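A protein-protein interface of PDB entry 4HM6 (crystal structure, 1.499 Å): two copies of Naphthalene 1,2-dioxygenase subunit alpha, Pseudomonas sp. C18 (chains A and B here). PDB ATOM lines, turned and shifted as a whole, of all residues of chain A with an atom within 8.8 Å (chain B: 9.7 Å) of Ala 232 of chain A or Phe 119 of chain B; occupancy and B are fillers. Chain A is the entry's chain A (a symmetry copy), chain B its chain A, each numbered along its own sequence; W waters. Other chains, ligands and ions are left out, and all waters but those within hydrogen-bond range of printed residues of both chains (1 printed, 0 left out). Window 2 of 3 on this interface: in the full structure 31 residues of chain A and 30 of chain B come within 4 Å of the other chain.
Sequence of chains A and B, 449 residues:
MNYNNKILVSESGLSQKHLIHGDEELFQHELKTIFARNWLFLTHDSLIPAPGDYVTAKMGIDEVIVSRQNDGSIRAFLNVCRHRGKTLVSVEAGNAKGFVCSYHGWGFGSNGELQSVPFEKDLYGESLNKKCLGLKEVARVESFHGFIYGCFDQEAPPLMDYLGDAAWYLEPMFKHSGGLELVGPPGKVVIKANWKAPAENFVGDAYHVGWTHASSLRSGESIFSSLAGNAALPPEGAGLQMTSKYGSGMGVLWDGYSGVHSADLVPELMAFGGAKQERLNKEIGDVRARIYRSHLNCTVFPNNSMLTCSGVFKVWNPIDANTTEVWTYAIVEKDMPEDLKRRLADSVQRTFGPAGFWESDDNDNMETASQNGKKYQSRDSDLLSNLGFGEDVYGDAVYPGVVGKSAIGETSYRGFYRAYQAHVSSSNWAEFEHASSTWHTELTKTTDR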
ATOM      1  N   ALA A 206       8.718 -20.215  26.973  1.00  0.00           N
ATOM      2  CA  ALA A 206      10.137 -20.129  27.288  1.00  0.00           C
ATOM      3  C   ALA A 206      10.707 -18.789  26.834  1.00  0.00           C
ATOM      4  O   ALA A 206      11.726 -18.340  27.358  1.00  0.00           O
ATOM      5  CB  ALA A 206      10.894 -21.276  26.657  1.00  0.00           C
ATOM      6  N   TYR A 207      10.048 -18.161  25.862  1.00  0.00           N
ATOM      7  CA  TYR A 207      10.523 -16.897  25.272  1.00  0.00           C
ATOM      8  C   TYR A 207      10.677 -15.814  26.336  1.00  0.00           C
ATOM      9  O   TYR A 207      11.628 -15.036  26.298  1.00  0.00           O
ATOM     10  CB  TYR A 207       9.532 -16.431  24.189  1.00  0.00           C
ATOM     11  CG  TYR A 207      10.003 -15.393  23.175  1.00  0.00           C
ATOM     12  CD1 TYR A 207      11.336 -15.006  23.068  1.00  0.00           C
ATOM     13  CD2 TYR A 207       9.085 -14.814  22.301  1.00  0.00           C
ATOM     14  CE1 TYR A 207      11.737 -14.056  22.119  1.00  0.00           C
ATOM     15  CE2 TYR A 207       9.471 -13.880  21.352  1.00  0.00           C
ATOM     16  CZ  TYR A 207      10.798 -13.503  21.266  1.00  0.00           C
ATOM     17  OH  TYR A 207      11.172 -12.571  20.322  1.00  0.00           O
ATOM     18  N   VAL A 209      11.453 -15.944  29.473  1.00  0.00           N
ATOM     19  CA  VAL A 209      12.307 -16.198  30.640  1.00  0.00           C
ATOM     20  C   VAL A 209      13.502 -15.256  30.775  1.00  0.00           C
ATOM     21  O   VAL A 209      13.692 -14.635  31.830  1.00  0.00           O
ATOM     22  CB  VAL A 209      12.764 -17.675  30.716  1.00  0.00           C
ATOM     23  CG1 VAL A 209      13.702 -17.885  31.913  1.00  0.00           C
ATOM     24  CG2 VAL A 209      11.553 -18.590  30.823  1.00  0.00           C
ATOM     25  N   GLY A 210      14.303 -15.131  29.719  1.00  0.00           N
ATOM     26  CA  GLY A 210      15.479 -14.273  29.778  1.00  0.00           C
ATOM     27  C   GLY A 210      15.179 -12.811  30.067  1.00  0.00           C
ATOM     28  O   GLY A 210      15.953 -12.127  30.746  1.00  0.00           O
ATOM     29  N   TRP A 211      14.048 -12.321  29.572  1.00  0.00           N
ATOM     30  CA  TRP A 211      13.717 -10.904  29.730  1.00  0.00           C
ATOM     31  C   TRP A 211      12.883 -10.631  30.978  1.00  0.00           C
ATOM     32  O   TRP A 211      13.267  -9.805  31.815  1.00  0.00           O
ATOM     33  CB  TRP A 211      13.022 -10.366  28.472  1.00  0.00           C
ATOM     34  CG  TRP A 211      13.064  -8.868  28.382  1.00  0.00           C
ATOM     35  CD1 TRP A 211      12.001  -8.020  28.434  1.00  0.00           C
ATOM     36  CD2 TRP A 211      14.230  -8.042  28.250  1.00  0.00           C
ATOM     37  NE1 TRP A 211      12.428  -6.718  28.337  1.00  0.00           N
ATOM     38  CE2 TRP A 211      13.794  -6.704  28.226  1.00  0.00           C
ATOM     39  CE3 TRP A 211      15.604  -8.304  28.160  1.00  0.00           C
ATOM     40  CZ2 TRP A 211      14.679  -5.624  28.107  1.00  0.00           C
ATOM     41  CZ3 TRP A 211      16.483  -7.229  28.039  1.00  0.00           C
ATOM     42  CH2 TRP A 211      16.018  -5.909  28.017  1.00  0.00           C
ATOM     43  N   LEU A 217      17.159 -14.365  37.387  1.00  0.00           N
ATOM     44  CA  LEU A 217      18.244 -15.130  36.784  1.00  0.00           C
ATOM     45  C   LEU A 217      19.608 -14.614  37.255  1.00  0.00           C
ATOM     46  O   LEU A 217      20.463 -15.397  37.668  1.00  0.00           O
ATOM     47  CB  LEU A 217      18.147 -15.059  35.262  1.00  0.00           C
ATOM     48  CG  LEU A 217      16.997 -15.847  34.636  1.00  0.00           C
ATOM     49  CD1 LEU A 217      16.752 -15.387  33.203  1.00  0.00           C
ATOM     50  CD2 LEU A 217      17.285 -17.342  34.681  1.00  0.00           C
ATOM     51  N   PHE A 224      19.793 -21.919  34.729  1.00  0.00           N
ATOM     52  CA  PHE A 224      19.320 -21.264  33.512  1.00  0.00           C
ATOM     53  C   PHE A 224      19.814 -19.813  33.448  1.00  0.00           C
ATOM     54  O   PHE A 224      19.390 -19.035  32.592  1.00  0.00           O
ATOM     55  CB  PHE A 224      17.790 -21.318  33.410  1.00  0.00           C
ATOM     56  CG  PHE A 224      17.212 -22.716  33.470  1.00  0.00           C
ATOM     57  CD1 PHE A 224      17.893 -23.794  32.928  1.00  0.00           C
ATOM     58  CD2 PHE A 224      15.979 -22.942  34.071  1.00  0.00           C
ATOM     59  CE1 PHE A 224      17.361 -25.072  32.988  1.00  0.00           C
ATOM     60  CE2 PHE A 224      15.437 -24.213  34.131  1.00  0.00           C
ATOM     61  CZ  PHE A 224      16.127 -25.281  33.588  1.00  0.00           C
ATOM     62  N   SER A 225      20.744 -19.469  34.336  1.00  0.00           N
ATOM     63  CA  SER A 225      21.163 -18.080  34.563  1.00  0.00           C
ATOM     64  C   SER A 225      21.835 -17.365  33.386  1.00  0.00           C
ATOM     65  O   SER A 225      21.914 -16.125  33.359  1.00  0.00           O
ATOM     66  CB  SER A 225      22.099 -18.023  35.770  1.00  0.00           C
ATOM     67  OG  SER A 225      22.389 -16.689  36.128  1.00  0.00           O
ATOM     68  N   SER A 226      22.338 -18.129  32.423  1.00  0.00           N
ATOM     69  CA  SER A 226      23.000 -17.532  31.266  1.00  0.00           C
ATOM     70  C   SER A 226      22.029 -16.729  30.409  1.00  0.00           C
ATOM     71  O   SER A 226      22.436 -15.997  29.502  1.00  0.00           O
ATOM     72  CB  SER A 226      23.639 -18.618  30.413  1.00  0.00           C
ATOM     73  OG  SER A 226      22.671 -19.565  29.982  1.00  0.00           O
ATOM     74  N   LEU A 227      20.744 -16.873  30.698  1.00  0.00           N
ATOM     75  CA  LEU A 227      19.712 -16.269  29.876  1.00  0.00           C
ATOM     76  C   LEU A 227      19.415 -14.828  30.289  1.00  0.00           C
ATOM     77  O   LEU A 227      18.751 -14.108  29.558  1.00  0.00           O
ATOM     78  CB  LEU A 227      18.434 -17.109  29.941  1.00  0.00           C
ATOM     79  CG  LEU A 227      18.525 -18.580  29.531  1.00  0.00           C
ATOM     80  CD1 LEU A 227      17.202 -19.291  29.786  1.00  0.00           C
ATOM     81  CD2 LEU A 227      18.916 -18.703  28.078  1.00  0.00           C
ATOM     82  N   ALA A 228      19.907 -14.412  31.456  1.00  0.00           N
ATOM     83  CA  ALA A 228      19.534 -13.115  32.041  1.00  0.00           C
ATOM     84  C   ALA A 228      19.651 -11.935  31.071  1.00  0.00           C
ATOM     85  O   ALA A 228      20.707 -11.710  30.469  1.00  0.00           O
ATOM     86  CB  ALA A 228      20.341 -12.840  33.321  1.00  0.00           C
ATOM     87  N   GLY A 229      18.557 -11.194  30.921  1.00  0.00           N
ATOM     88  CA  GLY A 229      18.528 -10.037  30.042  1.00  0.00           C
ATOM     89  C   GLY A 229      18.722 -10.365  28.575  1.00  0.00           C
ATOM     90  O   GLY A 229      19.215  -9.528  27.820  1.00  0.00           O
ATOM     91  N   ASN A 230      18.327 -11.569  28.162  1.00  0.00           N
ATOM     92  CA  ASN A 230      18.559 -12.034  26.789  1.00  0.00           C
ATOM     93  C   ASN A 230      20.019 -11.940  26.362  1.00  0.00           C
ATOM     94  O   ASN A 230      20.330 -11.637  25.208  1.00  0.00           O
ATOM     95  CB  ASN A 230      17.654 -11.309  25.785  1.00  0.00           C
ATOM     96  CG  ASN A 230      16.220 -11.769  25.873  1.00  0.00           C
ATOM     97  OD1 ASN A 230      15.940 -12.845  26.403  1.00  0.00           O
ATOM     98  ND2 ASN A 230      15.300 -10.962  25.357  1.00  0.00           N
ATOM     99  N   ALA A 231      20.910 -12.201  27.313  1.00  0.00           N
ATOM    100  CA  ALA A 231      22.343 -12.153  27.067  1.00  0.00           C
ATOM    101  C   ALA A 231      22.768 -13.312  26.181  1.00  0.00           C
ATOM    102  O   ALA A 231      23.783 -13.238  25.494  1.00  0.00           O
ATOM    103  CB  ALA A 231      23.087 -12.209  28.376  1.00  0.00           C
ATOM    104  N   ALA A 232      21.994 -14.391  26.218  1.00  0.00           N
ATOM    105  CA  ALA A 232      22.336 -15.587  25.468  1.00  0.00           C
ATOM    106  C   ALA A 232      21.096 -16.405  25.128  1.00  0.00           C
ATOM    107  O   ALA A 232      20.171 -16.523  25.934  1.00  0.00           O
ATOM    108  CB  ALA A 232      23.336 -16.429  26.254  1.00  0.00           C
ATOM    109  N   LEU A 233      21.081 -16.964  23.923  1.00  0.00           N
ATOM    110  CA  LEU A 233      20.005 -17.848  23.506  1.00  0.00           C
ATOM    111  C   LEU A 233      20.436 -19.275  23.813  1.00  0.00           C
ATOM    112  O   LEU A 233      21.608 -19.606  23.645  1.00  0.00           O
ATOM    113  CB  LEU A 233      19.747 -17.689  22.004  1.00  0.00           C
ATOM    114  CG  LEU A 233      18.488 -18.350  21.433  1.00  0.00           C
ATOM    115  CD1 LEU A 233      17.231 -17.711  21.996  1.00  0.00           C
ATOM    116  CD2 LEU A 233      18.482 -18.283  19.915  1.00  0.00           C
ATOM    117  N   PRO A 234      19.504 -20.115  24.293  1.00  0.00           N
ATOM    118  CA  PRO A 234      19.788 -21.546  24.430  1.00  0.00           C
ATOM    119  C   PRO A 234      20.279 -22.096  23.100  1.00  0.00           C
ATOM    120  O   PRO A 234      19.799 -21.675  22.049  1.00  0.00           O
ATOM    121  CB  PRO A 234      18.418 -22.139  24.762  1.00  0.00           C
ATOM    122  CG  PRO A 234      17.694 -21.033  25.439  1.00  0.00           C
ATOM    123  CD  PRO A 234      18.150 -19.773  24.763  1.00  0.00           C
ATOM    124  N   PRO A 235      21.243 -23.020  23.139  1.00  0.00           N
ATOM    125  CA  PRO A 235      21.793 -23.594  21.909  1.00  0.00           C
ATOM    126  C   PRO A 235      20.749 -24.410  21.156  1.00  0.00           C
ATOM    127  O   PRO A 235      19.708 -24.725  21.733  1.00  0.00           O
ATOM    128  CB  PRO A 235      22.896 -24.516  22.428  1.00  0.00           C
ATOM    129  CG  PRO A 235      22.545 -24.812  23.826  1.00  0.00           C
ATOM    130  CD  PRO A 235      21.856 -23.596  24.347  1.00  0.00           C
ATOM    131  N   LEU A 387       4.743 -18.036  16.728  1.00  0.00           N
ATOM    132  CA  LEU A 387       6.164 -18.390  16.713  1.00  0.00           C
ATOM    133  C   LEU A 387       6.349 -19.892  16.517  1.00  0.00           C
ATOM    134  O   LEU A 387       5.831 -20.697  17.298  1.00  0.00           O
ATOM    135  CB  LEU A 387       6.856 -17.920  17.997  1.00  0.00           C
ATOM    136  CG  LEU A 387       8.322 -18.293  18.177  1.00  0.00           C
ATOM    137  CD1 LEU A 387       9.128 -17.861  16.973  1.00  0.00           C
ATOM    138  CD2 LEU A 387       8.863 -17.664  19.455  1.00  0.00           C
ATOM    139  N   ILE A 408      12.414 -22.803  22.307  1.00  0.00           N
ATOM    140  CA  ILE A 408      11.588 -21.604  22.423  1.00  0.00           C
ATOM    141  C   ILE A 408      10.626 -21.473  21.252  1.00  0.00           C
ATOM    142  O   ILE A 408      11.048 -21.430  20.100  1.00  0.00           O
ATOM    143  CB  ILE A 408      12.460 -20.338  22.475  1.00  0.00           C
ATOM    144  CG1 ILE A 408      13.354 -20.365  23.718  1.00  0.00           C
ATOM    145  CG2 ILE A 408      11.581 -19.081  22.444  1.00  0.00           C
ATOM    146  CD1 ILE A 408      14.394 -19.273  23.745  1.00  0.00           C
ATOM    147  N   HIS B 104       8.212 -10.185  26.674  1.00  0.00           N
ATOM    148  CA  HIS B 104       9.162 -10.887  25.806  1.00  0.00           C
ATOM    149  C   HIS B 104      10.158  -9.966  25.091  1.00  0.00           C
ATOM    150  O   HIS B 104      10.895 -10.408  24.215  1.00  0.00           O
ATOM    151  CB  HIS B 104       8.444 -11.798  24.791  1.00  0.00           C
ATOM    152  CG  HIS B 104       7.354 -12.637  25.387  1.00  0.00           C
ATOM    153  ND1 HIS B 104       6.079 -12.163  25.604  1.00  0.00           N
ATOM    154  CD2 HIS B 104       7.349 -13.923  25.805  1.00  0.00           C
ATOM    155  CE1 HIS B 104       5.331 -13.118  26.124  1.00  0.00           C
ATOM    156  NE2 HIS B 104       6.080 -14.196  26.263  1.00  0.00           N
ATOM    157  N   GLY B 105      10.190  -8.692  25.463  1.00  0.00           N
ATOM    158  CA  GLY B 105      11.256  -7.818  25.003  1.00  0.00           C
ATOM    159  C   GLY B 105      11.107  -7.211  23.622  1.00  0.00           C
ATOM    160  O   GLY B 105      12.088  -6.689  23.076  1.00  0.00           O
ATOM    161  N   TRP B 106       9.906  -7.273  23.048  1.00  0.00           N
ATOM    162  CA  TRP B 106       9.671  -6.628  21.755  1.00  0.00           C
ATOM    163  C   TRP B 106       9.906  -5.128  21.872  1.00  0.00           C
ATOM    164  O   TRP B 106       9.487  -4.499  22.854  1.00  0.00           O
ATOM    165  CB  TRP B 106       8.254  -6.884  21.245  1.00  0.00           C
ATOM    166  CG  TRP B 106       8.028  -8.252  20.667  1.00  0.00           C
ATOM    167  CD1 TRP B 106       8.741  -9.384  20.920  1.00  0.00           C
ATOM    168  CD2 TRP B 106       6.999  -8.623  19.735  1.00  0.00           C
ATOM    169  NE1 TRP B 106       8.216 -10.441  20.205  1.00  0.00           N
ATOM    170  CE2 TRP B 106       7.147  -9.998  19.470  1.00  0.00           C
ATOM    171  CE3 TRP B 106       5.959  -7.921  19.106  1.00  0.00           C
ATOM    172  CZ2 TRP B 106       6.304 -10.693  18.597  1.00  0.00           C
ATOM    173  CZ3 TRP B 106       5.117  -8.617  18.231  1.00  0.00           C
ATOM    174  CH2 TRP B 106       5.300  -9.989  17.987  1.00  0.00           C
ATOM    175  N   GLY B 107      10.576  -4.554  20.876  1.00  0.00           N
ATOM    176  CA  GLY B 107      10.938  -3.145  20.927  1.00  0.00           C
ATOM    177  C   GLY B 107      10.231  -2.323  19.870  1.00  0.00           C
ATOM    178  O   GLY B 107      10.381  -2.573  18.665  1.00  0.00           O
ATOM    179  N   SER B 116      12.357  -4.102  16.786  1.00  0.00           N
ATOM    180  CA  SER B 116      13.216  -5.215  17.168  1.00  0.00           C
ATOM    181  C   SER B 116      12.441  -6.284  17.900  1.00  0.00           C
ATOM    182  O   SER B 116      11.527  -5.998  18.667  1.00  0.00           O
ATOM    183  CB  SER B 116      14.382  -4.739  18.031  1.00  0.00           C
ATOM    184  OG  SER B 116      13.931  -4.274  19.284  1.00  0.00           O
ATOM    185  N   VAL B 117      12.827  -7.525  17.646  1.00  0.00           N
ATOM    186  CA  VAL B 117      12.237  -8.678  18.290  1.00  0.00           C
ATOM    187  C   VAL B 117      13.426  -9.519  18.749  1.00  0.00           C
ATOM    188  O   VAL B 117      14.298  -9.830  17.943  1.00  0.00           O
ATOM    189  CB  VAL B 117      11.335  -9.432  17.273  1.00  0.00           C
ATOM    190  CG1 VAL B 117      11.172 -10.868  17.647  1.00  0.00           C
ATOM    191  CG2 VAL B 117       9.976  -8.738  17.148  1.00  0.00           C
ATOM    192  N   PRO B 118      13.501  -9.843  20.053  1.00  0.00           N
ATOM    193  CA  PRO B 118      14.683 -10.582  20.522  1.00  0.00           C
ATOM    194  C   PRO B 118      14.887 -11.890  19.773  1.00  0.00           C
ATOM    195  O   PRO B 118      13.934 -12.655  19.607  1.00  0.00           O
ATOM    196  CB  PRO B 118      14.371 -10.851  21.998  1.00  0.00           C
ATOM    197  CG  PRO B 118      13.466  -9.726  22.389  1.00  0.00           C
ATOM    198  CD  PRO B 118      12.609  -9.469  21.165  1.00  0.00           C
ATOM    199  N   PHE B 119      16.113 -12.105  19.297  1.00  0.00           N
ATOM    200  CA  PHE B 119      16.501 -13.317  18.577  1.00  0.00           C
ATOM    201  C   PHE B 119      15.617 -13.597  17.372  1.00  0.00           C
ATOM    202  O   PHE B 119      15.315 -14.752  17.078  1.00  0.00           O
ATOM    203  CB  PHE B 119      16.511 -14.523  19.523  1.00  0.00           C
ATOM    204  CG  PHE B 119      17.305 -14.299  20.779  1.00  0.00           C
ATOM    205  CD1 PHE B 119      18.685 -14.165  20.727  1.00  0.00           C
ATOM    206  CD2 PHE B 119      16.673 -14.243  22.012  1.00  0.00           C
ATOM    207  CE1 PHE B 119      19.423 -13.963  21.890  1.00  0.00           C
ATOM    208  CE2 PHE B 119      17.400 -14.048  23.175  1.00  0.00           C
ATOM    209  CZ  PHE B 119      18.775 -13.906  23.113  1.00  0.00           C
ATOM    210  N   GLU B 120      15.219 -12.541  16.666  1.00  0.00           N
ATOM    211  CA  GLU B 120      14.258 -12.684  15.577  1.00  0.00           C
ATOM    212  C   GLU B 120      14.711 -13.693  14.529  1.00  0.00           C
ATOM    213  O   GLU B 120      13.943 -14.576  14.136  1.00  0.00           O
ATOM    214  CB  GLU B 120      13.965 -11.332  14.922  1.00  0.00           C
ATOM    215  CG  GLU B 120      12.956 -11.427  13.786  1.00  0.00           C
ATOM    216  CD  GLU B 120      12.698 -10.103  13.089  1.00  0.00           C
ATOM    217  OE1 GLU B 120      13.366  -9.100  13.413  1.00  0.00           O
ATOM    218  OE2 GLU B 120      11.819 -10.076  12.205  1.00  0.00           O
ATOM    219  N   LYS B 121      15.963 -13.584  14.100  1.00  0.00           N
ATOM    220  CA  LYS B 121      16.489 -14.471  13.068  1.00  0.00           C
ATOM    221  C   LYS B 121      16.421 -15.947  13.481  1.00  0.00           C
ATOM    222  O   LYS B 121      16.007 -16.804  12.698  1.00  0.00           O
ATOM    223  CB  LYS B 121      17.928 -14.078  12.729  1.00  0.00           C
ATOM    224  CG  LYS B 121      18.601 -14.968  11.687  1.00  0.00           C
ATOM    225  CD  LYS B 121      17.768 -15.094  10.423  1.00  0.00           C
ATOM    226  CE  LYS B 121      18.649 -15.448   9.233  1.00  0.00           C
ATOM    227  NZ  LYS B 121      19.648 -14.367   8.992  1.00  0.00           N
ATOM    228  N   ASP B 122      16.810 -16.232  14.719  1.00  0.00           N
ATOM    229  CA  ASP B 122      16.870 -17.608  15.199  1.00  0.00           C
ATOM    230  C   ASP B 122      15.488 -18.198  15.465  1.00  0.00           C
ATOM    231  O   ASP B 122      15.294 -19.411  15.352  1.00  0.00           O
ATOM    232  CB  ASP B 122      17.709 -17.685  16.474  1.00  0.00           C
ATOM    233  CG  ASP B 122      19.199 -17.786  16.193  1.00  0.00           C
ATOM    234  OD1 ASP B 122      19.600 -18.667  15.405  1.00  0.00           O
ATOM    235  OD2 ASP B 122      19.967 -16.984  16.763  1.00  0.00           O
ATOM    236  N   LEU B 123      14.536 -17.341  15.829  1.00  0.00           N
ATOM    237  CA  LEU B 123      13.210 -17.792  16.243  1.00  0.00           C
ATOM    238  C   LEU B 123      12.178 -17.687  15.130  1.00  0.00           C
ATOM    239  O   LEU B 123      11.501 -18.664  14.802  1.00  0.00           O
ATOM    240  CB  LEU B 123      12.737 -16.992  17.456  1.00  0.00           C
ATOM    241  CG  LEU B 123      13.604 -17.138  18.711  1.00  0.00           C
ATOM    242  CD1 LEU B 123      13.081 -16.259  19.833  1.00  0.00           C
ATOM    243  CD2 LEU B 123      13.662 -18.590  19.162  1.00  0.00           C
ATOM    244  N   TYR B 124      12.052 -16.496  14.560  1.00  0.00           N
ATOM    245  CA  TYR B 124      11.050 -16.252  13.526  1.00  0.00           C
ATOM    246  C   TYR B 124      11.598 -16.419  12.118  1.00  0.00           C
ATOM    247  O   TYR B 124      10.826 -16.565  11.167  1.00  0.00           O
ATOM    248  CB  TYR B 124      10.462 -14.846  13.666  1.00  0.00           C
ATOM    249  CG  TYR B 124       9.624 -14.649  14.910  1.00  0.00           C
ATOM    250  CD1 TYR B 124       8.273 -14.976  14.920  1.00  0.00           C
ATOM    251  CD2 TYR B 124      10.187 -14.139  16.077  1.00  0.00           C
ATOM    252  CE1 TYR B 124       7.498 -14.792  16.056  1.00  0.00           C
ATOM    253  CE2 TYR B 124       9.427 -13.967  17.214  1.00  0.00           C
ATOM    254  CZ  TYR B 124       8.081 -14.291  17.197  1.00  0.00           C
ATOM    255  OH  TYR B 124       7.327 -14.107  18.335  1.00  0.00           O
ATOM    256  N   GLY B 125      12.920 -16.395  11.977  1.00  0.00           N
ATOM    257  CA  GLY B 125      13.517 -16.378  10.654  1.00  0.00           C
ATOM    258  C   GLY B 125      13.094 -15.107   9.938  1.00  0.00           C
ATOM    259  O   GLY B 125      13.206 -14.012  10.493  1.00  0.00           O
ATOM    260  N   GLU B 126      12.591 -15.250   8.714  1.00  0.00           N
ATOM    261  CA  GLU B 126      12.100 -14.107   7.948  1.00  0.00           C
ATOM    262  C   GLU B 126      10.573 -14.026   7.965  1.00  0.00           C
ATOM    263  O   GLU B 126       9.974 -13.252   7.211  1.00  0.00           O
ATOM    264  CB  GLU B 126      12.591 -14.198   6.502  1.00  0.00           C
ATOM    265  CG  GLU B 126      14.098 -14.343   6.371  1.00  0.00           C
ATOM    266  CD  GLU B 126      14.836 -13.065   6.712  1.00  0.00           C
ATOM    267  OE1 GLU B 126      14.253 -11.981   6.505  1.00  0.00           O
ATOM    268  OE2 GLU B 126      15.990 -13.142   7.186  1.00  0.00           O
ATOM    269  N   SER B 127       9.946 -14.820   8.829  1.00  0.00           N
ATOM    270  CA  SER B 127       8.500 -15.034   8.759  1.00  0.00           C
ATOM    271  C   SER B 127       7.661 -14.004   9.510  1.00  0.00           C
ATOM    272  O   SER B 127       6.449 -13.935   9.319  1.00  0.00           O
ATOM    273  CB  SER B 127       8.149 -16.428   9.273  1.00  0.00           C
ATOM    274  OG  SER B 127       8.358 -16.505  10.673  1.00  0.00           O
ATOM    275  N   LEU B 128       8.289 -13.211  10.371  1.00  0.00           N
ATOM    276  CA  LEU B 128       7.534 -12.229  11.140  1.00  0.00           C
ATOM    277  C   LEU B 128       7.398 -10.934  10.349  1.00  0.00           C
ATOM    278  O   LEU B 128       8.398 -10.293  10.035  1.00  0.00           O
ATOM    279  CB  LEU B 128       8.212 -11.961  12.484  1.00  0.00           C
ATOM    280  CG  LEU B 128       7.392 -11.151  13.485  1.00  0.00           C
ATOM    281  CD1 LEU B 128       6.146 -11.922  13.886  1.00  0.00           C
ATOM    282  CD2 LEU B 128       8.222 -10.796  14.699  1.00  0.00           C
ATOM    283  N   LYS B 130       6.972  -7.606  10.653  1.00  0.00           N
ATOM    284  CA  LYS B 130       6.999  -6.515  11.625  1.00  0.00           C
ATOM    285  C   LYS B 130       6.287  -5.267  11.114  1.00  0.00           C
ATOM    286  O   LYS B 130       5.765  -4.483  11.904  1.00  0.00           O
ATOM    287  CB  LYS B 130       8.438  -6.179  12.031  1.00  0.00           C
ATOM    288  CG  LYS B 130       9.176  -7.334  12.702  1.00  0.00           C
ATOM    289  CD  LYS B 130      10.515  -6.903  13.309  1.00  0.00           C
ATOM    290  CE  LYS B 130      11.469  -6.377  12.246  1.00  0.00           C
ATOM    291  NZ  LYS B 130      11.740  -7.410  11.200  1.00  0.00           N
HETATM  292  O   HOH W   1      12.507 -12.300  25.154  1.00  0.00           O
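The backbone carbonyl oxygen (O) of Pro 118 of chain B sits at hydrogen-bond distance from the side-chain hydroxyl (OH) of Tyr 207 of chain A, 2.9 Å away.
O of Tyr 124 of chain B lies within hydrogen-bond range of OG of Ser 127 of chain B (2.5 Å).
Among the printed residues, merely in contact across the chains: Tyr 207 of chain A with Val 117 of chain B, Leu 387 of chain A with Leu 123 of chain B, Tyr 207 of chain A with Leu 123 of chain B, Asn 230 of chain A with Phe 119 of chain B, Asn 230 of chain A with Pro 118 of chain B, Leu 233 of chain A with Phe 119 of chain B, Trp 211 of chain A with Gly 105 of chain B, Leu 233 of chain A with Asp 122 of chain B, Leu 387 of chain A with Tyr 124 of chain B, Tyr 207 of chain A with Trp 106 of chain B, Tyr 207 of chain A with His 104 of chain B, Tyr 207 of chain A with Tyr 124 of chain B, Ile 408 of chain A with Leu 123 of chain B and Ala 232 of chain A with Phe 119 of chain B.
No residue of chain B comes within 4 Å of Leu 227 of chain A. No residue of chain B comes within 4 Å of Ala 231 of chain A. Of chain B, only Phe 119 (3.96 Å) comes within 4 Å of Ala 232 of chain A. Pro 235 of chain A touches none of the printed residues of chain B. Printed residues of chain B within 4 Å of Ile 408 of chain A: Leu 123. Of the printed residues of chain A, His 104 of chain B touches Tyr 207 (3.7 Å). Phe 119 of chain B touches just these residues of chain A: Asn 230 (3.5 Å), Ala 232 (3.96 Å) and Leu 233 (3.5 Å). The nearest residue of chain B that does not touch Ala 232 of chain A is Asp 122 of chain B (8.5 Å). The nearest printed residue of chain A that does not touch Asp 122 of chain B is Leu 387 of chain A (6.5 Å).
Hydrophobic or aromatic side chains of chain A within 4 Å of the printed part of chain B: Tyr 207, Trp 211, Leu 233, Leu 387 and Ile 408. Of the 18 printed residues of chain B, 9 touch a printed residue of chain A. Hydrophobic or aromatic side chains of chain B within 4 Å of the printed part of chain A: His 104, Trp 106, Val 117, Pro 118, Phe 119, Leu 123 and Tyr 124. Along chain B the printed residues that touch a printed residue of chain A span positions 104 to 124. Among the printed residues, 15 pairs touch across the chains. Among the printed residues, no Asp or Glu carboxylate lies within 4 Å of a Lys or Arg side-chain nitrogen of the other chain.
No position is printed for both chains.
Water W1 lies within hydrogen-bond range of O of His 104 of chain B (2.7 Å), O of Tyr 207 of chain A (3.1 Å) and ND2 of Asn 230 of chain A (3.1 Å).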
